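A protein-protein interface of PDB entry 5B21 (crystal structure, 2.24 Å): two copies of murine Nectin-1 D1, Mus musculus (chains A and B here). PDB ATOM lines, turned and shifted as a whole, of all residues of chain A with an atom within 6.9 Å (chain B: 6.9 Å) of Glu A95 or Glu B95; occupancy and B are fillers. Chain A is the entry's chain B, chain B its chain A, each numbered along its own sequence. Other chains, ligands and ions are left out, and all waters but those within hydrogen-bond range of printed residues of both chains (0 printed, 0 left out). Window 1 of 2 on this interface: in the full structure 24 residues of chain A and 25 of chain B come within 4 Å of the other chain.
OE1 of Glu A105 lies within salt-bridge range of NZ of Lys B45.
OG1 of Thr B36 sits at hydrogen-bond distance from OD1 of Asn A103, at 3.5 Å.
NE2 of Gln B34 sits at hydrogen-bond distance from OD1 of Asn A103 (3.3 Å).
The side-chain carboxylate (OE1) of Glu A95 sits at hydrogen-bond distance from the side-chain amide nitrogen (ND2) of Asn B103 (2.4 Å).
OE1 of Glu B105 is in salt-bridge range of NZ of Lys A45 (3.7 Å).
OE2 of Glu B95 sits close to OE1 of Glu A95 (2.8 Å).
The side-chain amide nitrogen (ND2) of Asn A103 lies within hydrogen-bond range of the side-chain carboxylate (OE2) of Glu B95, at 3.0 Å.
O of Thr B98 lies close to OE1 of Gln A34, 3.3 Å away.
The side-chain amide oxygen of Gln B38 sits at hydrogen-bond distance from the side-chain amino group of Lys B45 (3.4 Å).
The backbone NH (N) of Ala B97 sits at hydrogen-bond distance from the backbone carbonyl oxygen (O) of Gln B34 (3.0 Å).
OE2 of Glu B95 is in hydrogen-bond range of ND2 of Asn B103.
O of Glu A95 is in hydrogen-bond range of N of Thr A36.
NE2 of Gln B34 sits at hydrogen-bond distance from OG1 of Thr B36 (2.9 Å).
The backbone carbonyl oxygen of Ile A93 is in hydrogen-bond range of the backbone NH of Gln A38.
Among the printed residues, merely in contact across the chains: Val A2 with Gln B38 (3.5 Å), Val A2 with Lys B45 (3.5 Å), Gln A34 with Ala B97 (3.7 Å), Thr A36 with Asn B103 (3.6 Å), Gln A38 with Asn B103 (3.8 Å) and Asn A103 with Gln B38 (3.9 Å).
Of chain B, only Glu B95 (2.8 Å) and Asn B103 (2.4 Å) come within 4 Å of Glu A95.
Glu B95 touches just these residues of chain A: Glu A95 and Asn A103.
Printed residues of chain B within 4 Å of Asn A103: Gln B34 (3.3 Å), Thr B36 (3.5 Å), Gln B38 (3.9 Å) and Glu B95 (3.0 Å).
Of the printed residues of chain B, Thr A36 touches Asn B103 (3.6 Å).
Printed residues of chain B within 4 Å of Lys A45: Glu B105.
Of the printed residues of chain A, Asn B103 touches Thr A36, Gln A38 and Glu A95.
Of the printed residues of chain B, Glu A105 touches Lys B45.
The nearest residue of chain B that does not touch Glu A95 is Gln B38 (5.1 Å).
Hydrophobic or aromatic side chains of chain B within 4 Å of the printed part of chain A: Ala B97.
Along chain B the printed residues that touch a printed residue of chain A span positions 34 to 105.
Of the 17 printed residues of chain A, 8 touch a printed residue of chain B.
Among the printed residues, Asp or Glu carboxylates within 4 Å of a Lys or Arg side-chain nitrogen of the other chain: Lys A45 with Glu B105 and Glu A105 with Lys B45.
Thr A36 touches Asn B103, and with the chains exchanged Asn A103 touches Thr B36.
Gln A38 touches Asn B103, and with the chains exchanged Asn A103 touches Gln B38.
Lys A45 touches Glu B105, and with the chains exchanged Glu A105 touches Lys B45.
Asn A103 touches Gln B34, but with the chains exchanged Gln A34 does not touch Asn B103 (4.6 Å).
Positions printed for both chains: 21, 34, 35, 36, 37, 38, 45, 93, 94, 95, 96, 97, 103, 104, 105 and 106.
Of the 14 pairs that touch across the chains among the printed residues, 9 have their exchanged pair printed and touching as well.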
ATOM      1  N   VAL A   2     -17.041  -5.710 -27.898  1.00  0.00           N
ATOM      2  CA  VAL A   2     -17.023  -5.557 -26.450  1.00  0.00           C
ATOM      3  C   VAL A   2     -17.110  -6.902 -25.733  1.00  0.00           C
ATOM      4  O   VAL A   2     -16.314  -7.194 -24.840  1.00  0.00           O
ATOM      5  CB  VAL A   2     -18.175  -4.654 -25.974  1.00  0.00           C
ATOM      6  CG1 VAL A   2     -18.216  -4.586 -24.452  1.00  0.00           C
ATOM      7  CG2 VAL A   2     -18.039  -3.259 -26.581  1.00  0.00           C
ATOM      8  N   CYS A  21     -11.449 -15.184 -15.531  1.00  0.00           N
ATOM      9  CA  CYS A  21     -11.506 -13.927 -16.257  1.00  0.00           C
ATOM     10  C   CYS A  21     -10.120 -13.292 -16.313  1.00  0.00           C
ATOM     11  O   CYS A  21      -9.603 -12.818 -15.301  1.00  0.00           O
ATOM     12  CB  CYS A  21     -12.505 -12.976 -15.599  1.00  0.00           C
ATOM     13  SG  CYS A  21     -12.794 -11.444 -16.494  1.00  0.00           S
ATOM     14  N   GLN A  34     -10.705  -0.992 -13.845  1.00  0.00           N
ATOM     15  CA  GLN A  34     -11.422  -1.866 -12.922  1.00  0.00           C
ATOM     16  C   GLN A  34     -11.809  -3.204 -13.544  1.00  0.00           C
ATOM     17  O   GLN A  34     -12.021  -3.308 -14.753  1.00  0.00           O
ATOM     18  CB  GLN A  34     -12.683  -1.173 -12.400  1.00  0.00           C
ATOM     19  CG  GLN A  34     -12.520  -0.514 -11.042  1.00  0.00           C
ATOM     20  CD  GLN A  34     -13.827   0.019 -10.492  1.00  0.00           C
ATOM     21  OE1 GLN A  34     -13.863   0.614  -9.416  1.00  0.00           O
ATOM     22  NE2 GLN A  34     -14.912  -0.195 -11.229  1.00  0.00           N
ATOM     23  N   VAL A  35     -11.895  -4.224 -12.697  1.00  0.00           N
ATOM     24  CA  VAL A  35     -12.454  -5.513 -13.075  1.00  0.00           C
ATOM     25  C   VAL A  35     -13.739  -5.707 -12.282  1.00  0.00           C
ATOM     26  O   VAL A  35     -13.750  -5.528 -11.069  1.00  0.00           O
ATOM     27  CB  VAL A  35     -11.482  -6.672 -12.793  1.00  0.00           C
ATOM     28  CG1 VAL A  35     -11.911  -7.918 -13.549  1.00  0.00           C
ATOM     29  CG2 VAL A  35     -10.065  -6.278 -13.175  1.00  0.00           C
ATOM     30  N   THR A  36     -14.824  -6.063 -12.958  1.00  0.00           N
ATOM     31  CA  THR A  36     -16.123  -6.111 -12.300  1.00  0.00           C
ATOM     32  C   THR A  36     -16.931  -7.356 -12.649  1.00  0.00           C
ATOM     33  O   THR A  36     -17.400  -7.514 -13.776  1.00  0.00           O
ATOM     34  CB  THR A  36     -16.963  -4.866 -12.648  1.00  0.00           C
ATOM     35  OG1 THR A  36     -16.236  -3.682 -12.292  1.00  0.00           O
ATOM     36  CG2 THR A  36     -18.284  -4.887 -11.896  1.00  0.00           C
ATOM     37  N   TRP A  37     -17.083  -8.236 -11.666  1.00  0.00           N
ATOM     38  CA  TRP A  37     -17.969  -9.384 -11.770  1.00  0.00           C
ATOM     39  C   TRP A  37     -19.411  -8.993 -11.465  1.00  0.00           C
ATOM     40  O   TRP A  37     -19.700  -8.411 -10.413  1.00  0.00           O
ATOM     41  CB  TRP A  37     -17.527 -10.498 -10.823  1.00  0.00           C
ATOM     42  CG  TRP A  37     -16.381 -11.309 -11.328  1.00  0.00           C
ATOM     43  CD1 TRP A  37     -15.065 -11.170 -10.993  1.00  0.00           C
ATOM     44  CD2 TRP A  37     -16.445 -12.393 -12.256  1.00  0.00           C
ATOM     45  NE1 TRP A  37     -14.305 -12.101 -11.657  1.00  0.00           N
ATOM     46  CE2 TRP A  37     -15.134 -12.870 -12.445  1.00  0.00           C
ATOM     47  CE3 TRP A  37     -17.487 -13.016 -12.954  1.00  0.00           C
ATOM     48  CZ2 TRP A  37     -14.830 -13.929 -13.291  1.00  0.00           C
ATOM     49  CZ3 TRP A  37     -17.187 -14.068 -13.798  1.00  0.00           C
ATOM     50  CH2 TRP A  37     -15.870 -14.513 -13.959  1.00  0.00           C
ATOM     51  N   GLN A  38     -20.299  -9.320 -12.401  1.00  0.00           N
ATOM     52  CA  GLN A  38     -21.734  -9.104 -12.260  1.00  0.00           C
ATOM     53  C   GLN A  38     -22.484 -10.392 -12.586  1.00  0.00           C
ATOM     54  O   GLN A  38     -22.045 -11.169 -13.434  1.00  0.00           O
ATOM     55  CB  GLN A  38     -22.214  -7.984 -13.185  1.00  0.00           C
ATOM     56  CG  GLN A  38     -21.347  -6.739 -13.192  1.00  0.00           C
ATOM     57  CD  GLN A  38     -21.700  -5.799 -14.328  1.00  0.00           C
ATOM     58  OE1 GLN A  38     -22.581  -4.950 -14.196  1.00  0.00           O
ATOM     59  NE2 GLN A  38     -21.013  -5.950 -15.456  1.00  0.00           N
ATOM     60  N   LYS A  45     -29.029  -7.357 -14.448  1.00  0.00           N
ATOM     61  CA  LYS A  45     -27.698  -7.624 -13.913  1.00  0.00           C
ATOM     62  C   LYS A  45     -27.573  -7.183 -12.457  1.00  0.00           C
ATOM     63  O   LYS A  45     -28.416  -6.446 -11.945  1.00  0.00           O
ATOM     64  CB  LYS A  45     -26.636  -6.929 -14.767  1.00  0.00           C
ATOM     65  CG  LYS A  45     -26.617  -7.381 -16.217  1.00  0.00           C
ATOM     66  CD  LYS A  45     -26.021  -6.316 -17.127  1.00  0.00           C
ATOM     67  CE  LYS A  45     -24.577  -6.009 -16.763  1.00  0.00           C
ATOM     68  NZ  LYS A  45     -23.990  -4.984 -17.670  1.00  0.00           N
ATOM     69  N   ILE A  93     -20.815 -12.205 -15.847  1.00  0.00           N
ATOM     70  CA  ILE A  93     -20.114 -11.236 -16.683  1.00  0.00           C
ATOM     71  C   ILE A  93     -18.921 -10.619 -15.959  1.00  0.00           C
ATOM     72  O   ILE A  93     -19.085  -9.960 -14.936  1.00  0.00           O
ATOM     73  CB  ILE A  93     -21.054 -10.096 -17.130  1.00  0.00           C
ATOM     74  CG1 ILE A  93     -22.372 -10.656 -17.669  1.00  0.00           C
ATOM     75  CG2 ILE A  93     -20.369  -9.211 -18.162  1.00  0.00           C
ATOM     76  CD1 ILE A  93     -22.224 -11.444 -18.946  1.00  0.00           C
ATOM     77  N   CYS A  94     -17.724 -10.828 -16.495  1.00  0.00           N
ATOM     78  CA  CYS A  94     -16.526 -10.208 -15.939  1.00  0.00           C
ATOM     79  C   CYS A  94     -16.053  -9.080 -16.849  1.00  0.00           C
ATOM     80  O   CYS A  94     -15.569  -9.326 -17.949  1.00  0.00           O
ATOM     81  CB  CYS A  94     -15.417 -11.243 -15.750  1.00  0.00           C
ATOM     82  SG  CYS A  94     -13.899 -10.583 -15.026  1.00  0.00           S
ATOM     83  N   GLU A  95     -16.185  -7.842 -16.386  1.00  0.00           N
ATOM     84  CA  GLU A  95     -15.932  -6.689 -17.241  1.00  0.00           C
ATOM     85  C   GLU A  95     -14.650  -5.932 -16.899  1.00  0.00           C
ATOM     86  O   GLU A  95     -14.418  -5.565 -15.752  1.00  0.00           O
ATOM     87  CB  GLU A  95     -17.116  -5.726 -17.176  1.00  0.00           C
ATOM     88  CG  GLU A  95     -17.009  -4.557 -18.133  1.00  0.00           C
ATOM     89  CD  GLU A  95     -17.954  -3.433 -17.774  1.00  0.00           C
ATOM     90  OE1 GLU A  95     -17.778  -2.839 -16.690  1.00  0.00           O
ATOM     91  OE2 GLU A  95     -18.871  -3.147 -18.570  1.00  0.00           O
ATOM     92  N   PHE A  96     -13.826  -5.695 -17.912  1.00  0.00           N
ATOM     93  CA  PHE A  96     -12.650  -4.847 -17.771  1.00  0.00           C
ATOM     94  C   PHE A  96     -12.938  -3.445 -18.290  1.00  0.00           C
ATOM     95  O   PHE A  96     -13.279  -3.268 -19.461  1.00  0.00           O
ATOM     96  CB  PHE A  96     -11.453  -5.436 -18.520  1.00  0.00           C
ATOM     97  CG  PHE A  96     -10.843  -6.630 -17.849  1.00  0.00           C
ATOM     98  CD1 PHE A  96      -9.816  -6.475 -16.933  1.00  0.00           C
ATOM     99  CD2 PHE A  96     -11.284  -7.908 -18.144  1.00  0.00           C
ATOM    100  CE1 PHE A  96      -9.245  -7.572 -16.319  1.00  0.00           C
ATOM    101  CE2 PHE A  96     -10.716  -9.008 -17.533  1.00  0.00           C
ATOM    102  CZ  PHE A  96      -9.697  -8.840 -16.618  1.00  0.00           C
ATOM    103  N   ALA A  97     -12.804  -2.455 -17.416  1.00  0.00           N
ATOM    104  CA  ALA A  97     -12.946  -1.060 -17.816  1.00  0.00           C
ATOM    105  C   ALA A  97     -11.583  -0.494 -18.198  1.00  0.00           C
ATOM    106  O   ALA A  97     -10.750  -0.227 -17.333  1.00  0.00           O
ATOM    107  CB  ALA A  97     -13.574  -0.244 -16.699  1.00  0.00           C
ATOM    108  N   ASN A 103     -14.485  -0.735 -22.815  1.00  0.00           N
ATOM    109  CA  ASN A 103     -14.698  -1.884 -21.945  1.00  0.00           C
ATOM    110  C   ASN A 103     -14.725  -3.217 -22.691  1.00  0.00           C
ATOM    111  O   ASN A 103     -15.300  -3.327 -23.773  1.00  0.00           O
ATOM    112  CB  ASN A 103     -15.998  -1.708 -21.155  1.00  0.00           C
ATOM    113  CG  ASN A 103     -15.919  -0.571 -20.150  1.00  0.00           C
ATOM    114  OD1 ASN A 103     -15.057   0.301 -20.249  1.00  0.00           O
ATOM    115  ND2 ASN A 103     -16.820  -0.579 -19.175  1.00  0.00           N
ATOM    116  N   ARG A 104     -14.084  -4.222 -22.099  1.00  0.00           N
ATOM    117  CA  ARG A 104     -14.107  -5.584 -22.625  1.00  0.00           C
ATOM    118  C   ARG A 104     -14.740  -6.528 -21.611  1.00  0.00           C
ATOM    119  O   ARG A 104     -14.166  -6.767 -20.553  1.00  0.00           O
ATOM    120  CB  ARG A 104     -12.696  -6.078 -22.952  1.00  0.00           C
ATOM    121  CG  ARG A 104     -12.121  -5.631 -24.283  1.00  0.00           C
ATOM    122  CD  ARG A 104     -10.812  -6.368 -24.535  1.00  0.00           C
ATOM    123  NE  ARG A 104      -9.993  -5.755 -25.575  1.00  0.00           N
ATOM    124  CZ  ARG A 104      -8.739  -6.110 -25.837  1.00  0.00           C
ATOM    125  NH1 ARG A 104      -8.163  -7.077 -25.134  1.00  0.00           N
ATOM    126  NH2 ARG A 104      -8.060  -5.503 -26.800  1.00  0.00           N
ATOM    127  N   GLU A 105     -15.907  -7.079 -21.925  1.00  0.00           N
ATOM    128  CA  GLU A 105     -16.566  -7.977 -20.981  1.00  0.00           C
ATOM    129  C   GLU A 105     -16.578  -9.432 -21.449  1.00  0.00           C
ATOM    130  O   GLU A 105     -17.040  -9.748 -22.545  1.00  0.00           O
ATOM    131  CB  GLU A 105     -17.997  -7.501 -20.704  1.00  0.00           C
ATOM    132  CG  GLU A 105     -18.855  -7.277 -21.937  1.00  0.00           C
ATOM    133  CD  GLU A 105     -20.250  -6.798 -21.588  1.00  0.00           C
ATOM    134  OE1 GLU A 105     -20.371  -5.751 -20.917  1.00  0.00           O
ATOM    135  OE2 GLU A 105     -21.227  -7.471 -21.981  1.00  0.00           O
ATOM    136  N   SER A 106     -16.048 -10.311 -20.604  1.00  0.00           N
ATOM    137  CA  SER A 106     -16.103 -11.749 -20.835  1.00  0.00           C
ATOM    138  C   SER A 106     -17.390 -12.319 -20.249  1.00  0.00           C
ATOM    139  O   SER A 106     -17.849 -11.886 -19.193  1.00  0.00           O
ATOM    140  CB  SER A 106     -14.883 -12.446 -20.230  1.00  0.00           C
ATOM    141  OG  SER A 106     -13.689 -12.033 -20.871  1.00  0.00           O
ATOM    142  N   CYS B  21     -26.770  11.814 -19.454  1.00  0.00           N
ATOM    143  CA  CYS B  21     -26.293  10.744 -18.588  1.00  0.00           C
ATOM    144  C   CYS B  21     -25.604  11.328 -17.361  1.00  0.00           C
ATOM    145  O   CYS B  21     -24.587  12.013 -17.479  1.00  0.00           O
ATOM    146  CB  CYS B  21     -25.337   9.821 -19.349  1.00  0.00           C
ATOM    147  SG  CYS B  21     -24.747   8.408 -18.393  1.00  0.00           S
ATOM    148  N   GLN B  34     -14.551   5.810 -13.944  1.00  0.00           N
ATOM    149  CA  GLN B  34     -14.649   5.982 -15.391  1.00  0.00           C
ATOM    150  C   GLN B  34     -16.098   6.082 -15.867  1.00  0.00           C
ATOM    151  O   GLN B  34     -17.007   5.543 -15.238  1.00  0.00           O
ATOM    152  CB  GLN B  34     -13.945   4.824 -16.105  1.00  0.00           C
ATOM    153  CG  GLN B  34     -13.710   5.043 -17.590  1.00  0.00           C
ATOM    154  CD  GLN B  34     -13.037   3.859 -18.253  1.00  0.00           C
ATOM    155  OE1 GLN B  34     -11.846   3.618 -18.059  1.00  0.00           O
ATOM    156  NE2 GLN B  34     -13.799   3.109 -19.041  1.00  0.00           N
ATOM    157  N   VAL B  35     -16.303   6.787 -16.978  1.00  0.00           N
ATOM    158  CA  VAL B  35     -17.611   6.876 -17.622  1.00  0.00           C
ATOM    159  C   VAL B  35     -17.507   6.410 -19.073  1.00  0.00           C
ATOM    160  O   VAL B  35     -16.669   6.902 -19.827  1.00  0.00           O
ATOM    161  CB  VAL B  35     -18.171   8.309 -17.587  1.00  0.00           C
ATOM    162  CG1 VAL B  35     -19.579   8.340 -18.159  1.00  0.00           C
ATOM    163  CG2 VAL B  35     -18.154   8.855 -16.169  1.00  0.00           C
ATOM    164  N   THR B  36     -18.358   5.466 -19.462  1.00  0.00           N
ATOM    165  CA  THR B  36     -18.252   4.852 -20.783  1.00  0.00           C
ATOM    166  C   THR B  36     -19.574   4.848 -21.551  1.00  0.00           C
ATOM    167  O   THR B  36     -20.623   4.521 -20.998  1.00  0.00           O
ATOM    168  CB  THR B  36     -17.742   3.402 -20.675  1.00  0.00           C
ATOM    169  OG1 THR B  36     -16.619   3.350 -19.785  1.00  0.00           O
ATOM    170  CG2 THR B  36     -17.333   2.872 -22.042  1.00  0.00           C
ATOM    171  N   TRP B  37     -19.511   5.212 -22.829  1.00  0.00           N
ATOM    172  CA  TRP B  37     -20.676   5.168 -23.707  1.00  0.00           C
ATOM    173  C   TRP B  37     -20.594   3.988 -24.669  1.00  0.00           C
ATOM    174  O   TRP B  37     -19.564   3.765 -25.303  1.00  0.00           O
ATOM    175  CB  TRP B  37     -20.811   6.471 -24.498  1.00  0.00           C
ATOM    176  CG  TRP B  37     -21.665   7.501 -23.827  1.00  0.00           C
ATOM    177  CD1 TRP B  37     -21.237   8.565 -23.087  1.00  0.00           C
ATOM    178  CD2 TRP B  37     -23.095   7.567 -23.832  1.00  0.00           C
ATOM    179  NE1 TRP B  37     -22.313   9.289 -22.633  1.00  0.00           N
ATOM    180  CE2 TRP B  37     -23.467   8.696 -23.076  1.00  0.00           C
ATOM    181  CE3 TRP B  37     -24.101   6.779 -24.404  1.00  0.00           C
ATOM    182  CZ2 TRP B  37     -24.796   9.059 -22.876  1.00  0.00           C
ATOM    183  CZ3 TRP B  37     -25.421   7.140 -24.205  1.00  0.00           C
ATOM    184  CH2 TRP B  37     -25.756   8.269 -23.448  1.00  0.00           C
ATOM    185  N   GLN B  38     -21.686   3.236 -24.775  1.00  0.00           N
ATOM    186  CA  GLN B  38     -21.738   2.079 -25.661  1.00  0.00           C
ATOM    187  C   GLN B  38     -23.019   2.062 -26.491  1.00  0.00           C
ATOM    188  O   GLN B  38     -24.028   2.648 -26.103  1.00  0.00           O
ATOM    189  CB  GLN B  38     -21.628   0.782 -24.856  1.00  0.00           C
ATOM    190  CG  GLN B  38     -20.283   0.570 -24.184  1.00  0.00           C
ATOM    191  CD  GLN B  38     -20.251  -0.684 -23.333  1.00  0.00           C
ATOM    192  OE1 GLN B  38     -21.218  -1.002 -22.640  1.00  0.00           O
ATOM    193  NE2 GLN B  38     -19.140  -1.408 -23.385  1.00  0.00           N
ATOM    194  N   LYS B  45     -22.397  -5.133 -28.743  1.00  0.00           N
ATOM    195  CA  LYS B  45     -22.003  -3.877 -28.115  1.00  0.00           C
ATOM    196  C   LYS B  45     -20.826  -3.239 -28.841  1.00  0.00           C
ATOM    197  O   LYS B  45     -19.981  -3.933 -29.407  1.00  0.00           O
ATOM    198  CB  LYS B  45     -21.648  -4.096 -26.643  1.00  0.00           C
ATOM    199  CG  LYS B  45     -22.816  -3.984 -25.683  1.00  0.00           C
ATOM    200  CD  LYS B  45     -22.328  -4.058 -24.245  1.00  0.00           C
ATOM    201  CE  LYS B  45     -23.456  -3.817 -23.257  1.00  0.00           C
ATOM    202  NZ  LYS B  45     -22.963  -3.832 -21.852  1.00  0.00           N
ATOM    203  N   ILE B  93     -25.939   2.940 -24.120  1.00  0.00           N
ATOM    204  CA  ILE B  93     -25.706   2.683 -22.705  1.00  0.00           C
ATOM    205  C   ILE B  93     -24.566   3.531 -22.152  1.00  0.00           C
ATOM    206  O   ILE B  93     -23.441   3.486 -22.654  1.00  0.00           O
ATOM    207  CB  ILE B  93     -25.386   1.193 -22.452  1.00  0.00           C
ATOM    208  CG1 ILE B  93     -26.350   0.295 -23.229  1.00  0.00           C
ATOM    209  CG2 ILE B  93     -25.433   0.880 -20.964  1.00  0.00           C
ATOM    210  CD1 ILE B  93     -25.661  -0.652 -24.187  1.00  0.00           C
ATOM    211  N   CYS B  94     -24.864   4.307 -21.117  1.00  0.00           N
ATOM    212  CA  CYS B  94     -23.853   5.092 -20.424  1.00  0.00           C
ATOM    213  C   CYS B  94     -23.533   4.441 -19.085  1.00  0.00           C
ATOM    214  O   CYS B  94     -24.390   4.358 -18.207  1.00  0.00           O
ATOM    215  CB  CYS B  94     -24.326   6.533 -20.221  1.00  0.00           C
ATOM    216  SG  CYS B  94     -23.150   7.589 -19.341  1.00  0.00           S
ATOM    217  N   GLU B  95     -22.296   3.981 -18.933  1.00  0.00           N
ATOM    218  CA  GLU B  95     -21.912   3.212 -17.755  1.00  0.00           C
ATOM    219  C   GLU B  95     -20.966   3.965 -16.824  1.00  0.00           C
ATOM    220  O   GLU B  95     -19.965   4.531 -17.262  1.00  0.00           O
ATOM    221  CB  GLU B  95     -21.260   1.896 -18.181  1.00  0.00           C
ATOM    222  CG  GLU B  95     -20.610   1.133 -17.041  1.00  0.00           C
ATOM    223  CD  GLU B  95     -19.666   0.055 -17.529  1.00  0.00           C
ATOM    224  OE1 GLU B  95     -19.923  -0.518 -18.609  1.00  0.00           O
ATOM    225  OE2 GLU B  95     -18.661  -0.211 -16.837  1.00  0.00           O
ATOM    226  N   PHE B  96     -21.295   3.962 -15.537  1.00  0.00           N
ATOM    227  CA  PHE B  96     -20.404   4.490 -14.511  1.00  0.00           C
ATOM    228  C   PHE B  96     -19.740   3.348 -13.748  1.00  0.00           C
ATOM    229  O   PHE B  96     -20.404   2.605 -13.025  1.00  0.00           O
ATOM    230  CB  PHE B  96     -21.160   5.392 -13.533  1.00  0.00           C
ATOM    231  CG  PHE B  96     -21.656   6.673 -14.138  1.00  0.00           C
ATOM    232  CD1 PHE B  96     -22.903   6.737 -14.734  1.00  0.00           C
ATOM    233  CD2 PHE B  96     -20.880   7.819 -14.094  1.00  0.00           C
ATOM    234  CE1 PHE B  96     -23.365   7.917 -15.284  1.00  0.00           C
ATOM    235  CE2 PHE B  96     -21.335   9.003 -14.644  1.00  0.00           C
ATOM    236  CZ  PHE B  96     -22.578   9.051 -15.241  1.00  0.00           C
ATOM    237  N   ALA B  97     -18.430   3.207 -13.918  1.00  0.00           N
ATOM    238  CA  ALA B  97     -17.665   2.237 -13.147  1.00  0.00           C
ATOM    239  C   ALA B  97     -17.274   2.847 -11.808  1.00  0.00           C
ATOM    240  O   ALA B  97     -16.492   3.793 -11.759  1.00  0.00           O
ATOM    241  CB  ALA B  97     -16.432   1.792 -13.915  1.00  0.00           C
ATOM    242  N   THR B  98     -17.826   2.315 -10.723  1.00  0.00           N
ATOM    243  CA  THR B  98     -17.598   2.888  -9.401  1.00  0.00           C
ATOM    244  C   THR B  98     -17.016   1.888  -8.407  1.00  0.00           C
ATOM    245  O   THR B  98     -17.100   0.675  -8.599  1.00  0.00           O
ATOM    246  CB  THR B  98     -18.900   3.460  -8.807  1.00  0.00           C
ATOM    247  OG1 THR B  98     -19.820   2.392  -8.548  1.00  0.00           O
ATOM    248  CG2 THR B  98     -19.536   4.458  -9.764  1.00  0.00           C
ATOM    249  N   GLY B 102     -19.543  -0.648  -7.730  1.00  0.00           N
ATOM    250  CA  GLY B 102     -19.505  -1.329  -9.010  1.00  0.00           C
ATOM    251  C   GLY B 102     -20.129  -0.525 -10.132  1.00  0.00           C
ATOM    252  O   GLY B 102     -20.144   0.704 -10.095  1.00  0.00           O
ATOM    253  N   ASN B 103     -20.653  -1.224 -11.132  1.00  0.00           N
ATOM    254  CA  ASN B 103     -21.216  -0.571 -12.307  1.00  0.00           C
ATOM    255  C   ASN B 103     -22.644  -0.076 -12.106  1.00  0.00           C
ATOM    256  O   ASN B 103     -23.508  -0.806 -11.621  1.00  0.00           O
ATOM    257  CB  ASN B 103     -21.171  -1.518 -13.507  1.00  0.00           C
ATOM    258  CG  ASN B 103     -19.768  -1.714 -14.044  1.00  0.00           C
ATOM    259  OD1 ASN B 103     -18.785  -1.369 -13.386  1.00  0.00           O
ATOM    260  ND2 ASN B 103     -19.667  -2.270 -15.245  1.00  0.00           N
ATOM    261  N   ARG B 104     -22.877   1.177 -12.483  1.00  0.00           N
ATOM    262  CA  ARG B 104     -24.218   1.744 -12.509  1.00  0.00           C
ATOM    263  C   ARG B 104     -24.464   2.377 -13.871  1.00  0.00           C
ATOM    264  O   ARG B 104     -23.808   3.354 -14.232  1.00  0.00           O
ATOM    265  CB  ARG B 104     -24.402   2.781 -11.404  1.00  0.00           C
ATOM    266  CG  ARG B 104     -25.727   3.518 -11.485  1.00  0.00           C
ATOM    267  CD  ARG B 104     -25.775   4.686 -10.521  1.00  0.00           C
ATOM    268  NE  ARG B 104     -27.067   5.367 -10.547  1.00  0.00           N
ATOM    269  CZ  ARG B 104     -27.398   6.310 -11.422  1.00  0.00           C
ATOM    270  NH1 ARG B 104     -26.534   6.688 -12.355  1.00  0.00           N
ATOM    271  NH2 ARG B 104     -28.598   6.874 -11.369  1.00  0.00           N
ATOM    272  N   GLU B 105     -25.405   1.825 -14.630  1.00  0.00           N
ATOM    273  CA  GLU B 105     -25.590   2.268 -16.005  1.00  0.00           C
ATOM    274  C   GLU B 105     -26.986   2.805 -16.312  1.00  0.00           C
ATOM    275  O   GLU B 105     -27.958   2.541 -15.593  1.00  0.00           O
ATOM    276  CB  GLU B 105     -25.260   1.128 -16.971  1.00  0.00           C
ATOM    277  CG  GLU B 105     -26.199  -0.061 -16.893  1.00  0.00           C
ATOM    278  CD  GLU B 105     -25.773  -1.192 -17.809  1.00  0.00           C
ATOM    279  OE1 GLU B 105     -24.553  -1.359 -18.020  1.00  0.00           O
ATOM    280  OE2 GLU B 105     -26.655  -1.911 -18.323  1.00  0.00           O
ATOM    281  N   SER B 106     -27.053   3.568 -17.398  1.00  0.00           N
ATOM    282  CA  SER B 106     -28.287   4.156 -17.896  1.00  0.00           C
ATOM    283  C   SER B 106     -28.483   3.765 -19.357  1.00  0.00           C
ATOM    284  O   SER B 106     -27.563   3.885 -20.163  1.00  0.00           O
ATOM    285  CB  SER B 106     -28.253   5.678 -17.754  1.00  0.00           C
ATOM    286  OG  SER B 106     -27.984   6.062 -16.417  1.00  0.00           O
